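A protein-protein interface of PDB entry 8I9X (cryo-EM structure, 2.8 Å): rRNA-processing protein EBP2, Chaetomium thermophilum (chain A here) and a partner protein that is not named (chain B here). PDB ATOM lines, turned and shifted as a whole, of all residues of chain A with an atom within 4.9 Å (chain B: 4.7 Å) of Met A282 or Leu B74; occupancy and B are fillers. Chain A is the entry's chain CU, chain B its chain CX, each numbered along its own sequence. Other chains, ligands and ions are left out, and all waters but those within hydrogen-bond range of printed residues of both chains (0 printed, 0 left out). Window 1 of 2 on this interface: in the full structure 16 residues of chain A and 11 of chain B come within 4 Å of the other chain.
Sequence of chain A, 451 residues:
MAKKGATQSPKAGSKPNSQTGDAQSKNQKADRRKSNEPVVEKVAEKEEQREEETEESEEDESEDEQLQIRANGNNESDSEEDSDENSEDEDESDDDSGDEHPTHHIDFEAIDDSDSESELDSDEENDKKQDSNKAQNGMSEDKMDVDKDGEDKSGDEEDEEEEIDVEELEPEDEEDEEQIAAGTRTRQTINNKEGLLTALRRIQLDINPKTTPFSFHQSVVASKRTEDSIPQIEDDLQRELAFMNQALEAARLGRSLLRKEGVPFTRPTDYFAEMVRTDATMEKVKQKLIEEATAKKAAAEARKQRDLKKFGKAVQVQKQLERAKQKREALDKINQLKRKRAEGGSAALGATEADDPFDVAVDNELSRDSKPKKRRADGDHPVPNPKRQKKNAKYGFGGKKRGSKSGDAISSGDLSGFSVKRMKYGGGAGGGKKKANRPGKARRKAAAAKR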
ATOM      1  N   ARG A 277       8.636  13.526 -23.487  1.00  0.00           N
ATOM      2  CA  ARG A 277       9.534  13.078 -22.435  1.00  0.00           C
ATOM      3  C   ARG A 277       9.633  14.165 -21.376  1.00  0.00           C
ATOM      4  O   ARG A 277       9.761  15.348 -21.706  1.00  0.00           O
ATOM      5  CB  ARG A 277      10.913  12.747 -22.998  1.00  0.00           C
ATOM      6  CG  ARG A 277      10.916  11.656 -24.049  1.00  0.00           C
ATOM      7  CD  ARG A 277      12.272  11.571 -24.718  1.00  0.00           C
ATOM      8  NE  ARG A 277      13.210  10.771 -23.941  1.00  0.00           N
ATOM      9  CZ  ARG A 277      14.524  10.784 -24.111  1.00  0.00           C
ATOM     10  NH1 ARG A 277      15.095  11.549 -25.026  1.00  0.00           N
ATOM     11  NH2 ARG A 277      15.285  10.012 -23.342  1.00  0.00           N
ATOM     12  N   THR A 278       9.579  13.764 -20.111  1.00  0.00           N
ATOM     13  CA  THR A 278       9.405  14.715 -19.026  1.00  0.00           C
ATOM     14  C   THR A 278      10.710  15.437 -18.686  1.00  0.00           C
ATOM     15  O   THR A 278      11.813  15.026 -19.071  1.00  0.00           O
ATOM     16  CB  THR A 278       8.866  14.013 -17.782  1.00  0.00           C
ATOM     17  OG1 THR A 278       9.803  13.022 -17.346  1.00  0.00           O
ATOM     18  CG2 THR A 278       7.538  13.340 -18.090  1.00  0.00           C
ATOM     19  N   ASP A 279      10.557  16.535 -17.940  1.00  0.00           N
ATOM     20  CA  ASP A 279      11.710  17.283 -17.453  1.00  0.00           C
ATOM     21  C   ASP A 279      12.598  16.423 -16.571  1.00  0.00           C
ATOM     22  O   ASP A 279      13.820  16.585 -16.578  1.00  0.00           O
ATOM     23  CB  ASP A 279      11.250  18.517 -16.679  1.00  0.00           C
ATOM     24  CG  ASP A 279      10.928  19.686 -17.581  1.00  0.00           C
ATOM     25  OD1 ASP A 279       9.732  20.012 -17.713  1.00  0.00           O
ATOM     26  OD2 ASP A 279      11.865  20.280 -18.153  1.00  0.00           O
ATOM     27  N   ALA A 280      12.005  15.507 -15.803  1.00  0.00           N
ATOM     28  CA  ALA A 280      12.805  14.585 -15.006  1.00  0.00           C
ATOM     29  C   ALA A 280      13.665  13.698 -15.898  1.00  0.00           C
ATOM     30  O   ALA A 280      14.847  13.469 -15.614  1.00  0.00           O
ATOM     31  CB  ALA A 280      11.895  13.742 -14.115  1.00  0.00           C
ATOM     32  N   THR A 281      13.088  13.193 -16.990  1.00  0.00           N
ATOM     33  CA  THR A 281      13.850  12.343 -17.900  1.00  0.00           C
ATOM     34  C   THR A 281      14.982  13.117 -18.561  1.00  0.00           C
ATOM     35  O   THR A 281      16.110  12.618 -18.661  1.00  0.00           O
ATOM     36  CB  THR A 281      12.923  11.742 -18.954  1.00  0.00           C
ATOM     37  OG1 THR A 281      11.793  11.143 -18.309  1.00  0.00           O
ATOM     38  CG2 THR A 281      13.654  10.685 -19.759  1.00  0.00           C
ATOM     39  N   MET A 282      14.701  14.339 -19.022  1.00  0.00           N
ATOM     40  CA  MET A 282      15.771  15.194 -19.529  1.00  0.00           C
ATOM     41  C   MET A 282      16.832  15.483 -18.482  1.00  0.00           C
ATOM     42  O   MET A 282      18.018  15.545 -18.825  1.00  0.00           O
ATOM     43  CB  MET A 282      15.190  16.495 -20.080  1.00  0.00           C
ATOM     44  CG  MET A 282      14.250  16.271 -21.232  1.00  0.00           C
ATOM     45  SD  MET A 282      15.167  15.377 -22.502  1.00  0.00           S
ATOM     46  CE  MET A 282      14.124  13.965 -22.776  1.00  0.00           C
ATOM     47  N   GLU A 283      16.444  15.650 -17.220  1.00  0.00           N
ATOM     48  CA  GLU A 283      17.428  15.833 -16.165  1.00  0.00           C
ATOM     49  C   GLU A 283      18.326  14.613 -16.011  1.00  0.00           C
ATOM     50  O   GLU A 283      19.540  14.766 -15.858  1.00  0.00           O
ATOM     51  CB  GLU A 283      16.728  16.150 -14.845  1.00  0.00           C
ATOM     52  CG  GLU A 283      17.674  16.404 -13.685  1.00  0.00           C
ATOM     53  CD  GLU A 283      18.521  17.648 -13.876  1.00  0.00           C
ATOM     54  OE1 GLU A 283      18.089  18.565 -14.605  1.00  0.00           O
ATOM     55  OE2 GLU A 283      19.626  17.707 -13.297  1.00  0.00           O
ATOM     56  N   LYS A 284      17.759  13.406 -16.054  1.00  0.00           N
ATOM     57  CA  LYS A 284      18.599  12.212 -15.963  1.00  0.00           C
ATOM     58  C   LYS A 284      19.524  12.064 -17.168  1.00  0.00           C
ATOM     59  O   LYS A 284      20.685  11.668 -17.006  1.00  0.00           O
ATOM     60  CB  LYS A 284      17.748  10.954 -15.787  1.00  0.00           C
ATOM     61  CG  LYS A 284      16.529  11.129 -14.917  1.00  0.00           C
ATOM     62  CD  LYS A 284      16.000   9.796 -14.427  1.00  0.00           C
ATOM     63  CE  LYS A 284      14.504   9.861 -14.175  1.00  0.00           C
ATOM     64  NZ  LYS A 284      14.018   8.679 -13.411  1.00  0.00           N
ATOM     65  N   VAL A 285      19.036  12.360 -18.375  1.00  0.00           N
ATOM     66  CA  VAL A 285      19.915  12.324 -19.544  1.00  0.00           C
ATOM     67  C   VAL A 285      21.056  13.323 -19.389  1.00  0.00           C
ATOM     68  O   VAL A 285      22.224  13.000 -19.647  1.00  0.00           O
ATOM     69  CB  VAL A 285      19.118  12.576 -20.837  1.00  0.00           C
ATOM     70  CG1 VAL A 285      20.011  12.375 -22.046  1.00  0.00           C
ATOM     71  CG2 VAL A 285      17.934  11.640 -20.922  1.00  0.00           C
ATOM     72  N   LYS A 286      20.733  14.541 -18.950  1.00  0.00           N
ATOM     73  CA  LYS A 286      21.755  15.551 -18.710  1.00  0.00           C
ATOM     74  C   LYS A 286      22.766  15.068 -17.681  1.00  0.00           C
ATOM     75  O   LYS A 286      23.974  15.247 -17.852  1.00  0.00           O
ATOM     76  CB  LYS A 286      21.095  16.850 -18.250  1.00  0.00           C
ATOM     77  CG  LYS A 286      22.043  18.017 -18.066  1.00  0.00           C
ATOM     78  CD  LYS A 286      21.279  19.276 -17.689  1.00  0.00           C
ATOM     79  CE  LYS A 286      22.214  20.455 -17.492  1.00  0.00           C
ATOM     80  NZ  LYS A 286      21.474  21.692 -17.120  1.00  0.00           N
ATOM     81  N   LEU A 289      25.103  12.461 -19.084  1.00  0.00           N
ATOM     82  CA  LEU A 289      26.086  13.142 -19.920  1.00  0.00           C
ATOM     83  C   LEU A 289      27.157  13.811 -19.066  1.00  0.00           C
ATOM     84  O   LEU A 289      28.357  13.727 -19.370  1.00  0.00           O
ATOM     85  CB  LEU A 289      25.397  14.172 -20.814  1.00  0.00           C
ATOM     86  CG  LEU A 289      24.660  13.640 -22.041  1.00  0.00           C
ATOM     87  CD1 LEU A 289      23.706  14.685 -22.589  1.00  0.00           C
ATOM     88  CD2 LEU A 289      25.654  13.212 -23.099  1.00  0.00           C
ATOM     89  N   PRO B  72      25.735  18.685 -24.783  1.00  0.00           N
ATOM     90  CA  PRO B  72      24.723  19.196 -25.715  1.00  0.00           C
ATOM     91  C   PRO B  72      23.522  19.767 -24.975  1.00  0.00           C
ATOM     92  O   PRO B  72      23.181  19.337 -23.871  1.00  0.00           O
ATOM     93  CB  PRO B  72      24.339  17.956 -26.530  1.00  0.00           C
ATOM     94  CG  PRO B  72      25.524  17.063 -26.437  1.00  0.00           C
ATOM     95  CD  PRO B  72      26.077  17.280 -25.057  1.00  0.00           C
ATOM     96  N   GLN B  73      22.882  20.753 -25.596  1.00  0.00           N
ATOM     97  CA  GLN B  73      21.653  21.314 -25.056  1.00  0.00           C
ATOM     98  C   GLN B  73      20.490  20.364 -25.306  1.00  0.00           C
ATOM     99  O   GLN B  73      20.400  19.733 -26.362  1.00  0.00           O
ATOM    100  CB  GLN B  73      21.367  22.680 -25.679  1.00  0.00           C
ATOM    101  CG  GLN B  73      22.574  23.596 -25.731  1.00  0.00           C
ATOM    102  CD  GLN B  73      22.252  24.946 -26.332  1.00  0.00           C
ATOM    103  OE1 GLN B  73      21.265  25.583 -25.963  1.00  0.00           O
ATOM    104  NE2 GLN B  73      23.086  25.394 -27.261  1.00  0.00           N
ATOM    105  N   LEU B  74      19.596  20.269 -24.328  1.00  0.00           N
ATOM    106  CA  LEU B  74      18.502  19.311 -24.350  1.00  0.00           C
ATOM    107  C   LEU B  74      17.170  20.044 -24.421  1.00  0.00           C
ATOM    108  O   LEU B  74      16.953  21.027 -23.707  1.00  0.00           O
ATOM    109  CB  LEU B  74      18.543  18.419 -23.107  1.00  0.00           C
ATOM    110  CG  LEU B  74      19.754  17.493 -23.009  1.00  0.00           C
ATOM    111  CD1 LEU B  74      19.763  16.762 -21.679  1.00  0.00           C
ATOM    112  CD2 LEU B  74      19.777  16.511 -24.167  1.00  0.00           C
ATOM    113  N   ASN B  75      16.276  19.555 -25.277  1.00  0.00           N
ATOM    114  CA  ASN B  75      14.993  20.205 -25.518  1.00  0.00           C
ATOM    115  C   ASN B  75      13.993  19.764 -24.458  1.00  0.00           C
ATOM    116  O   ASN B  75      13.719  18.568 -24.312  1.00  0.00           O
ATOM    117  CB  ASN B  75      14.481  19.883 -26.920  1.00  0.00           C
ATOM    118  CG  ASN B  75      13.310  20.750 -27.328  1.00  0.00           C
ATOM    119  OD1 ASN B  75      13.147  21.864 -26.831  1.00  0.00           O
ATOM    120  ND2 ASN B  75      12.492  20.248 -28.243  1.00  0.00           N
ATOM    121  N   THR B  76      13.466  20.726 -23.711  1.00  0.00           N
ATOM    122  CA  THR B  76      12.507  20.466 -22.644  1.00  0.00           C
ATOM    123  C   THR B  76      11.339  21.429 -22.836  1.00  0.00           C
ATOM    124  O   THR B  76      11.173  22.046 -23.894  1.00  0.00           O
ATOM    125  CB  THR B  76      13.147  20.608 -21.256  1.00  0.00           C
ATOM    126  OG1 THR B  76      13.194  21.992 -20.889  1.00  0.00           O
ATOM    127  CG2 THR B  76      14.556  20.032 -21.234  1.00  0.00           C
ATOM    128  N   VAL B  80      15.014  24.876 -26.577  1.00  0.00           N
ATOM    129  CA  VAL B  80      16.412  25.168 -26.881  1.00  0.00           C
ATOM    130  C   VAL B  80      16.510  26.286 -27.911  1.00  0.00           C
ATOM    131  O   VAL B  80      17.429  27.112 -27.873  1.00  0.00           O
ATOM    132  CB  VAL B  80      17.144  23.900 -27.352  1.00  0.00           C
ATOM    133  CG1 VAL B  80      17.266  22.919 -26.218  1.00  0.00           C
ATOM    134  CG2 VAL B  80      16.407  23.257 -28.515  1.00  0.00           C
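Of the 11 printed residues of chain A, 3 touch a printed residue of chain B. Along chain B the printed residues that touch a printed residue of chain A span positions 74 to 76. Among the printed residues, 5 pairs touch across the chains. Among the printed residues, no Asp or Glu carboxylate lies within 4 Å of a Lys or Arg side-chain nitrogen of the other chain.
The side-chain carboxylate (OD2) of Asp A279 lies close to the side-chain hydroxyl (OG1) of Thr B76, at 3.5 Å.
Of chain B, only Leu B74, Asn B75 and Thr B76 come within 4 Å of Met A282. Leu B74 touches just these residues of chain A: Met A282 and Lys A286. Of the printed residues of chain B, Asp A279 touches Thr B76. Of the printed residues of chain B, Lys A286 touches Leu B74 (3.6 Å). The nearest printed residue of chain B that does not touch Met A282 is Gln B73 (7.8 Å). The nearest printed residue of chain B that does not touch Asp A279 is Asn B75 (6.7 Å).
Among the printed residues, pairs that only touch across the chains: Met A282 with Leu B74, Met A282 with Asn B75, Met A282 with Thr B76 and Lys A286 with Leu B74.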
